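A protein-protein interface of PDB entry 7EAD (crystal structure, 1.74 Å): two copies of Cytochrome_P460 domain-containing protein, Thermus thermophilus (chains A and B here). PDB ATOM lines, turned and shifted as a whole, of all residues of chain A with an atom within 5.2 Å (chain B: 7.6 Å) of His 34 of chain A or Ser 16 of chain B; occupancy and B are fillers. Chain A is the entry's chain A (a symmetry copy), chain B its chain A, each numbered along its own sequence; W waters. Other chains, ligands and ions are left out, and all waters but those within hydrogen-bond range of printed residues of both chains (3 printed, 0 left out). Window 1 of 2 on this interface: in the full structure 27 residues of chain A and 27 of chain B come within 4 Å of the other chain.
Of the 15 printed residues of chain B, 9 touch a printed residue of chain A. Hydrophobic or aromatic side chains of chain B within 4 Å of the printed part of chain A: His 13, Met 17, His 34 and Tyr 36. Printed residues of chain A that touch a printed residue of chain B: His 13, Lys 15, Ser 16, His 34, Tyr 36, Leu 64, Leu 73 and Glu 75. Among the printed residues, 16 pairs touch across the chains. Among the printed residues, Asp or Glu carboxylates within 4 Å of a Lys or Arg side-chain nitrogen of the other chain: Glu 75 of chain A with Arg 134 of chain B.
His 13 of chain A touches His 34 of chain B, and with the chains exchanged His 34 of chain A touches His 13 of chain B. His 13 of chain A touches Tyr 36 of chain B, and with the chains exchanged Tyr 36 of chain A touches His 13 of chain B. Ser 16 of chain A touches His 34 of chain B, and with the chains exchanged His 34 of chain A touches Ser 16 of chain B. Ser 16 of chain A touches Glu 75 of chain B, and with the chains exchanged Glu 75 of chain A touches Ser 16 of chain B.
Printed residues of chain B within 4 Å of Ser 16 of chain A: His 34 and Glu 75. Of the printed residues of chain B, His 34 of chain A touches His 13, Ser 16 and Arg 134. Of the printed residues of chain B, Glu 75 of chain A touches Lys 15, Ser 16 and Arg 134. Of the printed residues of chain A, His 13 of chain B touches His 34 and Tyr 36. Of the printed residues of chain A, Lys 15 of chain B touches Glu 75. Ser 16 of chain B touches just these residues of chain A: His 34 and Glu 75. Printed residues of chain A within 4 Å of Tyr 36 of chain B: His 13 (2.7 Å). Ser 131 of chain B touches none of the printed residues of chain A. The nearest residue of chain B that does not touch His 34 of chain A is His 34 of chain B (4.7 Å). The nearest printed residue of chain B that does not touch Leu 73 of chain A is Ser 16 of chain B (4.8 Å).
OH of Tyr 36 of chain A sits at hydrogen-bond distance from ND1 of His 13 of chain B, 2.7 Å away. The backbone NH (N) of Ser 16 of chain B sits at hydrogen-bond distance from the side-chain carboxylate (OE1) of Glu 75 of chain A (3.0 Å). The backbone carbonyl oxygen of Glu 18 of chain B is in hydrogen-bond range of the backbone NH of Leu 73 of chain A, 2.8 Å away. The side-chain hydroxyl (OH) of Tyr 36 of chain B is in hydrogen-bond range of a ring nitrogen (ND1) of His 13 of chain A (2.7 Å). OE1 of Glu 75 of chain B sits at hydrogen-bond distance from N of Ser 16 of chain A (3.0 Å). OE1 of Glu 75 of chain A lies within salt-bridge range of NE of Arg 134 of chain B (2.9 Å).
Water W1 lies within hydrogen-bond range of NH2 of Arg 134 of chain B (2.7 Å), OH of Tyr 36 of chain A (2.8 Å) and OD2 of Asp 62 of chain A (2.8 Å). Water W2 bridges O of Ser 16 of chain B and N of Glu 75 of chain A. Water W3 bridges the backbone carbonyl oxygen of Ser 16 of chain A (2.8 Å) and the backbone NH of Glu 75 of chain B (2.9 Å).
The backbone carbonyl oxygen (O) of Lys 15 of chain B is in hydrogen-bond range of a ring nitrogen (NE2) of His 13 of chain B, 3.2 Å away. O of Val 14 of chain B sits at hydrogen-bond distance from N of Arg 134 of chain B (3.0 Å). ND1 of His 34 of chain B is in hydrogen-bond range of OG of Ser 16 of chain B, 2.7 Å away. NE2 of His 13 of chain A is in hydrogen-bond range of OG of Ser 16 of chain A (2.6 Å). O of His 34 of chain A is in hydrogen-bond range of N of Asp 62 of chain A (2.8 Å). A ring nitrogen (NE2) of His 34 of chain A is in hydrogen-bond range of the side-chain carboxylate (OE2) of Glu 75 of chain A (2.8 Å).
His 13 of chain A touches His 34 of chain B. Lys 15 of chain A touches Glu 75 of chain B (CB to OE1, 3.4 Å). OG of Ser 16 of chain A touches CE1 of His 34 of chain B, 3.4 Å away. ND1 of His 34 of chain A touches CE1 of His 13 of chain B, 3.7 Å away. CE1 of His 34 of chain A touches OG of Ser 16 of chain B, at 3.4 Å. His 34 of chain A touches Arg 134 of chain B. NH2 of Arg 134 of chain B touches OH of Tyr 36 of chain A, at 3.96 Å. Leu 64 of chain A touches Arg 134 of chain B (CD1 to CZ, 3.6 Å). O of Leu 73 of chain A touches CA of Met 17 of chain B (3.5 Å). Glu 75 of chain A touches Lys 15 of chain B (OE1 to CB, 3.4 Å).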
ATOM      1  N   HIS A  13      -8.357  34.449   6.523  1.00  0.00           N
ATOM      2  CA  HIS A  13      -7.922  33.743   5.314  1.00  0.00           C
ATOM      3  C   HIS A  13      -7.470  34.753   4.257  1.00  0.00           C
ATOM      4  O   HIS A  13      -8.266  35.585   3.810  1.00  0.00           O
ATOM      5  CB  HIS A  13      -9.089  32.879   4.815  1.00  0.00           C
ATOM      6  CG  HIS A  13      -8.803  32.100   3.564  1.00  0.00           C
ATOM      7  ND1 HIS A  13      -9.793  31.751   2.671  1.00  0.00           N
ATOM      8  CD2 HIS A  13      -7.651  31.583   3.073  1.00  0.00           C
ATOM      9  CE1 HIS A  13      -9.265  31.058   1.675  1.00  0.00           C
ATOM     10  NE2 HIS A  13      -7.966  30.941   1.895  1.00  0.00           N
ATOM     11  N   LYS A  15      -5.504  34.018   1.132  1.00  0.00           N
ATOM     12  CA  LYS A  15      -5.636  33.466  -0.213  1.00  0.00           C
ATOM     13  C   LYS A  15      -5.423  31.962  -0.131  1.00  0.00           C
ATOM     14  O   LYS A  15      -5.013  31.427   0.902  1.00  0.00           O
ATOM     15  CB  LYS A  15      -4.630  34.085  -1.183  1.00  0.00           C
ATOM     16  CG  LYS A  15      -3.197  33.712  -0.851  1.00  0.00           C
ATOM     17  CD  LYS A  15      -2.210  34.234  -1.892  1.00  0.00           C
ATOM     18  CE  LYS A  15      -2.405  33.533  -3.236  1.00  0.00           C
ATOM     19  NZ  LYS A  15      -1.412  34.076  -4.224  1.00  0.00           N
ATOM     20  N   SER A  16      -5.695  31.290  -1.249  1.00  0.00           N
ATOM     21  CA  SER A  16      -5.413  29.873  -1.410  1.00  0.00           C
ATOM     22  C   SER A  16      -4.764  29.668  -2.769  1.00  0.00           C
ATOM     23  O   SER A  16      -4.890  30.507  -3.661  1.00  0.00           O
ATOM     24  CB  SER A  16      -6.679  29.020  -1.290  1.00  0.00           C
ATOM     25  OG  SER A  16      -7.333  29.282  -0.054  1.00  0.00           O
ATOM     26  N   LEU A  32      -2.482  21.752  -1.846  1.00  0.00           N
ATOM     27  CA  LEU A  32      -3.344  22.914  -1.691  1.00  0.00           C
ATOM     28  C   LEU A  32      -2.942  23.627  -0.411  1.00  0.00           C
ATOM     29  O   LEU A  32      -2.925  23.012   0.665  1.00  0.00           O
ATOM     30  CB  LEU A  32      -4.821  22.512  -1.631  1.00  0.00           C
ATOM     31  CG  LEU A  32      -5.841  23.629  -1.378  1.00  0.00           C
ATOM     32  CD1 LEU A  32      -5.877  24.669  -2.490  1.00  0.00           C
ATOM     33  CD2 LEU A  32      -7.228  23.028  -1.189  1.00  0.00           C
ATOM     34  N   HIS A  33      -2.618  24.914  -0.519  1.00  0.00           N
ATOM     35  CA  HIS A  33      -2.262  25.673   0.664  1.00  0.00           C
ATOM     36  C   HIS A  33      -3.172  26.883   0.849  1.00  0.00           C
ATOM     37  O   HIS A  33      -3.687  27.468  -0.109  1.00  0.00           O
ATOM     38  CB  HIS A  33      -0.771  26.089   0.658  1.00  0.00           C
ATOM     39  CG  HIS A  33      -0.416  27.175  -0.316  1.00  0.00           C
ATOM     40  ND1 HIS A  33       0.199  26.921  -1.524  1.00  0.00           N
ATOM     41  CD2 HIS A  33      -0.537  28.522  -0.233  1.00  0.00           C
ATOM     42  CE1 HIS A  33       0.423  28.063  -2.154  1.00  0.00           C
ATOM     43  NE2 HIS A  33      -0.020  29.050  -1.393  1.00  0.00           N
ATOM     44  N   HIS A  34      -3.398  27.212   2.115  1.00  0.00           N
ATOM     45  CA  HIS A  34      -4.145  28.384   2.535  1.00  0.00           C
ATOM     46  C   HIS A  34      -3.237  29.238   3.400  1.00  0.00           C
ATOM     47  O   HIS A  34      -2.502  28.713   4.235  1.00  0.00           O
ATOM     48  CB  HIS A  34      -5.376  28.021   3.356  1.00  0.00           C
ATOM     49  CG  HIS A  34      -6.241  26.982   2.721  1.00  0.00           C
ATOM     50  ND1 HIS A  34      -6.936  27.206   1.551  1.00  0.00           N
ATOM     51  CD2 HIS A  34      -6.510  25.706   3.086  1.00  0.00           C
ATOM     52  CE1 HIS A  34      -7.613  26.116   1.232  1.00  0.00           C
ATOM     53  NE2 HIS A  34      -7.373  25.193   2.148  1.00  0.00           N
ATOM     54  N   ILE A  35      -3.288  30.546   3.199  1.00  0.00           N
ATOM     55  CA  ILE A  35      -2.487  31.487   3.969  1.00  0.00           C
ATOM     56  C   ILE A  35      -3.412  32.215   4.933  1.00  0.00           C
ATOM     57  O   ILE A  35      -4.533  32.593   4.572  1.00  0.00           O
ATOM     58  CB  ILE A  35      -1.727  32.452   3.035  1.00  0.00           C
ATOM     59  CG1 ILE A  35      -0.624  31.666   2.320  1.00  0.00           C
ATOM     60  CG2 ILE A  35      -1.117  33.622   3.819  1.00  0.00           C
ATOM     61  CD1 ILE A  35      -0.051  32.331   1.072  1.00  0.00           C
ATOM     62  N   TYR A  36      -2.949  32.379   6.174  1.00  0.00           N
ATOM     63  CA  TYR A  36      -3.705  33.032   7.229  1.00  0.00           C
ATOM     64  C   TYR A  36      -2.826  34.085   7.877  1.00  0.00           C
ATOM     65  O   TYR A  36      -1.611  33.908   7.973  1.00  0.00           O
ATOM     66  CB  TYR A  36      -4.142  32.051   8.308  1.00  0.00           C
ATOM     67  CG  TYR A  36      -5.013  30.959   7.780  1.00  0.00           C
ATOM     68  CD1 TYR A  36      -6.390  31.119   7.713  1.00  0.00           C
ATOM     69  CD2 TYR A  36      -4.457  29.767   7.332  1.00  0.00           C
ATOM     70  CE1 TYR A  36      -7.196  30.113   7.205  1.00  0.00           C
ATOM     71  CE2 TYR A  36      -5.250  28.757   6.834  1.00  0.00           C
ATOM     72  CZ  TYR A  36      -6.617  28.932   6.773  1.00  0.00           C
ATOM     73  OH  TYR A  36      -7.401  27.913   6.270  1.00  0.00           O
ATOM     74  N   VAL A  60       0.750  32.336   8.446  1.00  0.00           N
ATOM     75  CA  VAL A  60       0.844  30.886   8.418  1.00  0.00           C
ATOM     76  C   VAL A  60       0.509  30.389   7.021  1.00  0.00           C
ATOM     77  O   VAL A  60      -0.524  30.753   6.444  1.00  0.00           O
ATOM     78  CB  VAL A  60      -0.068  30.217   9.463  1.00  0.00           C
ATOM     79  CG1 VAL A  60       0.043  28.706   9.324  1.00  0.00           C
ATOM     80  CG2 VAL A  60       0.317  30.684  10.884  1.00  0.00           C
ATOM     81  N   PHE A  61       1.402  29.577   6.486  1.00  0.00           N
ATOM     82  CA  PHE A  61       1.234  28.891   5.215  1.00  0.00           C
ATOM     83  C   PHE A  61       0.789  27.472   5.559  1.00  0.00           C
ATOM     84  O   PHE A  61       1.587  26.674   6.056  1.00  0.00           O
ATOM     85  CB  PHE A  61       2.570  28.948   4.473  1.00  0.00           C
ATOM     86  CG  PHE A  61       2.590  28.264   3.137  1.00  0.00           C
ATOM     87  CD1 PHE A  61       2.613  26.876   3.044  1.00  0.00           C
ATOM     88  CD2 PHE A  61       2.676  29.012   1.971  1.00  0.00           C
ATOM     89  CE1 PHE A  61       2.680  26.247   1.806  1.00  0.00           C
ATOM     90  CE2 PHE A  61       2.736  28.383   0.728  1.00  0.00           C
ATOM     91  CZ  PHE A  61       2.737  27.003   0.654  1.00  0.00           C
ATOM     92  N   ASP A  62      -0.500  27.173   5.352  1.00  0.00           N
ATOM     93  CA  ASP A  62      -1.089  25.893   5.743  1.00  0.00           C
ATOM     94  C   ASP A  62      -1.168  24.992   4.515  1.00  0.00           C
ATOM     95  O   ASP A  62      -1.946  25.258   3.597  1.00  0.00           O
ATOM     96  CB  ASP A  62      -2.474  26.095   6.360  1.00  0.00           C
ATOM     97  CG  ASP A  62      -2.946  24.877   7.124  1.00  0.00           C
ATOM     98  OD1 ASP A  62      -2.300  23.823   6.970  1.00  0.00           O
ATOM     99  OD2 ASP A  62      -3.959  24.962   7.864  1.00  0.00           O
ATOM    100  N   LEU A  63      -0.370  23.930   4.499  1.00  0.00           N
ATOM    101  CA  LEU A  63      -0.209  23.089   3.314  1.00  0.00           C
ATOM    102  C   LEU A  63      -0.964  21.778   3.494  1.00  0.00           C
ATOM    103  O   LEU A  63      -0.665  21.016   4.417  1.00  0.00           O
ATOM    104  CB  LEU A  63       1.265  22.796   3.054  1.00  0.00           C
ATOM    105  CG  LEU A  63       1.517  21.916   1.822  1.00  0.00           C
ATOM    106  CD1 LEU A  63       0.863  22.513   0.586  1.00  0.00           C
ATOM    107  CD2 LEU A  63       3.014  21.710   1.591  1.00  0.00           C
ATOM    108  N   LEU A  64      -1.889  21.494   2.581  1.00  0.00           N
ATOM    109  CA  LEU A  64      -2.682  20.274   2.633  1.00  0.00           C
ATOM    110  C   LEU A  64      -2.464  19.450   1.374  1.00  0.00           C
ATOM    111  O   LEU A  64      -2.210  19.991   0.294  1.00  0.00           O
ATOM    112  CB  LEU A  64      -4.176  20.576   2.764  1.00  0.00           C
ATOM    113  CG  LEU A  64      -4.663  21.603   3.787  1.00  0.00           C
ATOM    114  CD1 LEU A  64      -6.149  21.806   3.588  1.00  0.00           C
ATOM    115  CD2 LEU A  64      -4.348  21.161   5.204  1.00  0.00           C
ATOM    116  N   LEU A  73     -11.653  18.841  -6.471  1.00  0.00           N
ATOM    117  CA  LEU A  73     -10.434  18.911  -5.680  1.00  0.00           C
ATOM    118  C   LEU A  73     -10.850  18.990  -4.218  1.00  0.00           C
ATOM    119  O   LEU A  73     -11.562  19.920  -3.830  1.00  0.00           O
ATOM    120  CB  LEU A  73      -9.573  20.120  -6.057  1.00  0.00           C
ATOM    121  CG  LEU A  73      -8.295  20.227  -5.225  1.00  0.00           C
ATOM    122  CD1 LEU A  73      -7.396  19.034  -5.480  1.00  0.00           C
ATOM    123  CD2 LEU A  73      -7.561  21.535  -5.512  1.00  0.00           C
ATOM    124  N   GLU A  75      -9.759  18.766   0.023  1.00  0.00           N
ATOM    125  CA  GLU A  75      -8.679  18.928   0.982  1.00  0.00           C
ATOM    126  C   GLU A  75      -8.286  17.573   1.556  1.00  0.00           C
ATOM    127  O   GLU A  75      -9.120  16.859   2.120  1.00  0.00           O
ATOM    128  CB  GLU A  75      -9.099  19.901   2.079  1.00  0.00           C
ATOM    129  CG  GLU A  75      -9.402  21.298   1.521  1.00  0.00           C
ATOM    130  CD  GLU A  75      -9.934  22.261   2.570  1.00  0.00           C
ATOM    131  OE1 GLU A  75     -10.984  21.957   3.188  1.00  0.00           O
ATOM    132  OE2 GLU A  75      -9.298  23.321   2.763  1.00  0.00           O
ATOM    133  N   HIS B  13     -12.581  30.369   8.372  1.00  0.00           N
ATOM    134  CA  HIS B  13     -12.555  29.511   7.183  1.00  0.00           C
ATOM    135  C   HIS B  13     -12.880  28.069   7.577  1.00  0.00           C
ATOM    136  O   HIS B  13     -12.150  27.458   8.364  1.00  0.00           O
ATOM    137  CB  HIS B  13     -11.169  29.627   6.536  1.00  0.00           C
ATOM    138  CG  HIS B  13     -10.978  28.789   5.306  1.00  0.00           C
ATOM    139  ND1 HIS B  13      -9.743  28.307   4.926  1.00  0.00           N
ATOM    140  CD2 HIS B  13     -11.854  28.369   4.362  1.00  0.00           C
ATOM    141  CE1 HIS B  13      -9.865  27.618   3.803  1.00  0.00           C
ATOM    142  NE2 HIS B  13     -11.136  27.641   3.439  1.00  0.00           N
ATOM    143  N   VAL B  14     -13.969  27.519   7.035  1.00  0.00           N
ATOM    144  CA  VAL B  14     -14.428  26.173   7.410  1.00  0.00           C
ATOM    145  C   VAL B  14     -13.747  25.094   6.575  1.00  0.00           C
ATOM    146  O   VAL B  14     -13.194  24.126   7.110  1.00  0.00           O
ATOM    147  CB  VAL B  14     -15.965  26.089   7.268  1.00  0.00           C
ATOM    148  CG1 VAL B  14     -16.464  24.662   7.495  1.00  0.00           C
ATOM    149  CG2 VAL B  14     -16.625  27.059   8.208  1.00  0.00           C
ATOM    150  N   LYS B  15     -13.800  25.252   5.255  1.00  0.00           N
ATOM    151  CA  LYS B  15     -13.227  24.305   4.303  1.00  0.00           C
ATOM    152  C   LYS B  15     -13.193  24.971   2.936  1.00  0.00           C
ATOM    153  O   LYS B  15     -13.762  26.046   2.731  1.00  0.00           O
ATOM    154  CB  LYS B  15     -14.034  23.009   4.234  1.00  0.00           C
ATOM    155  CG  LYS B  15     -15.418  23.215   3.646  1.00  0.00           C
ATOM    156  CD  LYS B  15     -16.171  21.899   3.470  1.00  0.00           C
ATOM    157  CE  LYS B  15     -15.512  21.027   2.402  1.00  0.00           C
ATOM    158  NZ  LYS B  15     -16.288  19.749   2.262  1.00  0.00           N
ATOM    159  N   SER B  16     -12.526  24.301   1.996  1.00  0.00           N
ATOM    160  CA  SER B  16     -12.509  24.702   0.599  1.00  0.00           C
ATOM    161  C   SER B  16     -12.733  23.465  -0.254  1.00  0.00           C
ATOM    162  O   SER B  16     -12.522  22.339   0.199  1.00  0.00           O
ATOM    163  CB  SER B  16     -11.192  25.383   0.215  1.00  0.00           C
ATOM    164  OG  SER B  16     -10.940  26.488   1.076  1.00  0.00           O
ATOM    165  N   MET B  17     -13.109  23.697  -1.482  1.00  0.00           N
ATOM    166  CA  MET B  17     -13.344  22.627  -2.420  1.00  0.00           C
ATOM    167  C   MET B  17     -13.499  23.154  -3.836  1.00  0.00           C
ATOM    168  O   MET B  17     -14.071  24.149  -4.011  1.00  0.00           O
ATOM    169  CB  MET B  17     -14.610  21.878  -2.029  1.00  0.00           C
ATOM    170  CG  MET B  17     -14.863  20.580  -2.744  1.00  0.00           C
ATOM    171  SD  MET B  17     -16.474  19.860  -2.305  1.00  0.00           S
ATOM    172  CE  MET B  17     -16.296  18.260  -2.979  1.00  0.00           C
ATOM    173  N   GLU B  18     -12.893  22.502  -4.818  1.00  0.00           N
ATOM    174  CA  GLU B  18     -13.066  22.866  -6.218  1.00  0.00           C
ATOM    175  C   GLU B  18     -14.013  21.870  -6.867  1.00  0.00           C
ATOM    176  O   GLU B  18     -13.828  20.662  -6.731  1.00  0.00           O
ATOM    177  CB  GLU B  18     -11.742  22.882  -6.987  1.00  0.00           C
ATOM    178  CG  GLU B  18     -11.853  23.605  -8.327  1.00  0.00           C
ATOM    179  CD  GLU B  18     -10.937  23.041  -9.412  1.00  0.00           C
ATOM    180  OE1 GLU B  18     -10.091  22.169  -9.116  1.00  0.00           O
ATOM    181  OE2 GLU B  18     -11.066  23.485 -10.574  1.00  0.00           O
ATOM    182  N   LEU B  32     -13.786  27.208  -7.575  1.00  0.00           N
ATOM    183  CA  LEU B  32     -13.207  27.008  -6.255  1.00  0.00           C
ATOM    184  C   LEU B  32     -14.047  27.783  -5.254  1.00  0.00           C
ATOM    185  O   LEU B  32     -14.241  28.997  -5.412  1.00  0.00           O
ATOM    186  CB  LEU B  32     -11.751  27.482  -6.204  1.00  0.00           C
ATOM    187  CG  LEU B  32     -11.041  27.415  -4.846  1.00  0.00           C
ATOM    188  CD1 LEU B  32     -10.892  25.995  -4.318  1.00  0.00           C
ATOM    189  CD2 LEU B  32      -9.670  28.073  -4.949  1.00  0.00           C
ATOM    190  N   HIS B  33     -14.547  27.092  -4.231  1.00  0.00           N
ATOM    191  CA  HIS B  33     -15.325  27.769  -3.213  1.00  0.00           C
ATOM    192  C   HIS B  33     -14.718  27.584  -1.825  1.00  0.00           C
ATOM    193  O   HIS B  33     -14.077  26.573  -1.521  1.00  0.00           O
ATOM    194  CB  HIS B  33     -16.812  27.334  -3.235  1.00  0.00           C
ATOM    195  CG  HIS B  33     -17.078  25.950  -2.718  1.00  0.00           C
ATOM    196  ND1 HIS B  33     -17.301  24.874  -3.551  1.00  0.00           N
ATOM    197  CD2 HIS B  33     -17.217  25.481  -1.454  1.00  0.00           C
ATOM    198  CE1 HIS B  33     -17.545  23.796  -2.823  1.00  0.00           C
ATOM    199  NE2 HIS B  33     -17.493  24.137  -1.546  1.00  0.00           N
ATOM    200  N   HIS B  34     -14.892  28.614  -1.007  1.00  0.00           N
ATOM    201  CA  HIS B  34     -14.493  28.626   0.389  1.00  0.00           C
ATOM    202  C   HIS B  34     -15.729  28.886   1.231  1.00  0.00           C
ATOM    203  O   HIS B  34     -16.557  29.724   0.876  1.00  0.00           O
ATOM    204  CB  HIS B  34     -13.478  29.722   0.691  1.00  0.00           C
ATOM    205  CG  HIS B  34     -12.312  29.739  -0.243  1.00  0.00           C
ATOM    206  ND1 HIS B  34     -11.384  28.720  -0.291  1.00  0.00           N
ATOM    207  CD2 HIS B  34     -11.934  30.643  -1.176  1.00  0.00           C
ATOM    208  CE1 HIS B  34     -10.470  29.007  -1.203  1.00  0.00           C
ATOM    209  NE2 HIS B  34     -10.780  30.169  -1.752  1.00  0.00           N
ATOM    210  N   ILE B  35     -15.852  28.168   2.337  1.00  0.00           N
ATOM    211  CA  ILE B  35     -16.977  28.324   3.249  1.00  0.00           C
ATOM    212  C   ILE B  35     -16.477  29.038   4.496  1.00  0.00           C
ATOM    213  O   ILE B  35     -15.382  28.749   4.995  1.00  0.00           O
ATOM    214  CB  ILE B  35     -17.618  26.957   3.566  1.00  0.00           C
ATOM    215  CG1 ILE B  35     -18.343  26.458   2.313  1.00  0.00           C
ATOM    216  CG2 ILE B  35     -18.604  27.062   4.738  1.00  0.00           C
ATOM    217  CD1 ILE B  35     -18.674  24.969   2.295  1.00  0.00           C
ATOM    218  N   TYR B  36     -17.270  29.997   4.977  1.00  0.00           N
ATOM    219  CA  TYR B  36     -16.941  30.795   6.146  1.00  0.00           C
ATOM    220  C   TYR B  36     -18.127  30.781   7.093  1.00  0.00           C
ATOM    221  O   TYR B  36     -19.275  30.733   6.651  1.00  0.00           O
ATOM    222  CB  TYR B  36     -16.642  32.242   5.783  1.00  0.00           C
ATOM    223  CG  TYR B  36     -15.489  32.376   4.843  1.00  0.00           C
ATOM    224  CD1 TYR B  36     -14.191  32.486   5.323  1.00  0.00           C
ATOM    225  CD2 TYR B  36     -15.695  32.381   3.469  1.00  0.00           C
ATOM    226  CE1 TYR B  36     -13.120  32.592   4.450  1.00  0.00           C
ATOM    227  CE2 TYR B  36     -14.638  32.495   2.593  1.00  0.00           C
ATOM    228  CZ  TYR B  36     -13.354  32.601   3.086  1.00  0.00           C
ATOM    229  OH  TYR B  36     -12.302  32.713   2.198  1.00  0.00           O
ATOM    230  N   GLU B  75      -6.856  31.371  -7.640  1.00  0.00           N
ATOM    231  CA  GLU B  75      -8.161  31.973  -7.426  1.00  0.00           C
ATOM    232  C   GLU B  75      -8.452  32.985  -8.527  1.00  0.00           C
ATOM    233  O   GLU B  75      -7.686  33.929  -8.738  1.00  0.00           O
ATOM    234  CB  GLU B  75      -8.217  32.617  -6.044  1.00  0.00           C
ATOM    235  CG  GLU B  75      -8.022  31.587  -4.924  1.00  0.00           C
ATOM    236  CD  GLU B  75      -7.957  32.211  -3.539  1.00  0.00           C
ATOM    237  OE1 GLU B  75      -7.071  33.069  -3.307  1.00  0.00           O
ATOM    238  OE2 GLU B  75      -8.793  31.831  -2.690  1.00  0.00           O
ATOM    239  N   SER B 131     -21.140  20.975   4.759  1.00  0.00           N
ATOM    240  CA  SER B 131     -19.723  21.110   5.050  1.00  0.00           C
ATOM    241  C   SER B 131     -19.427  20.752   6.497  1.00  0.00           C
ATOM    242  O   SER B 131     -20.238  20.968   7.405  1.00  0.00           O
ATOM    243  CB  SER B 131     -19.252  22.532   4.781  1.00  0.00           C
ATOM    244  OG  SER B 131     -20.088  23.473   5.441  1.00  0.00           O
ATOM    245  N   ALA B 132     -18.250  20.171   6.695  1.00  0.00           N
ATOM    246  CA  ALA B 132     -17.679  19.909   8.008  1.00  0.00           C
ATOM    247  C   ALA B 132     -16.451  20.792   8.180  1.00  0.00           C
ATOM    248  O   ALA B 132     -15.715  21.042   7.216  1.00  0.00           O
ATOM    249  CB  ALA B 132     -17.303  18.431   8.156  1.00  0.00           C
ATOM    250  N   ARG B 134     -12.853  21.625   8.755  1.00  0.00           N
ATOM    251  CA  ARG B 134     -11.659  20.831   8.527  1.00  0.00           C
ATOM    252  C   ARG B 134     -10.536  21.323   9.420  1.00  0.00           C
ATOM    253  O   ARG B 134     -10.110  22.484   9.287  1.00  0.00           O
ATOM    254  CB  ARG B 134     -11.223  20.888   7.077  1.00  0.00           C
ATOM    255  CG  ARG B 134      -9.939  20.104   6.919  1.00  0.00           C
ATOM    256  CD  ARG B 134      -9.111  20.578   5.771  1.00  0.00           C
ATOM    257  NE  ARG B 134      -9.212  22.003   5.503  1.00  0.00           N
ATOM    258  CZ  ARG B 134      -8.494  22.955   6.088  1.00  0.00           C
ATOM    259  NH1 ARG B 134      -7.611  22.667   7.037  1.00  0.00           N
ATOM    260  NH2 ARG B 134      -8.677  24.207   5.714  1.00  0.00           N
HETATM  261  O   HOH W   1      -6.469  25.358   6.761  1.00  0.00           O
HETATM  262  O   HOH W   2     -12.492  19.598   0.487  1.00  0.00           O
HETATM  263  O   HOH W   3      -4.524  31.905  -6.009  1.00  0.00           O
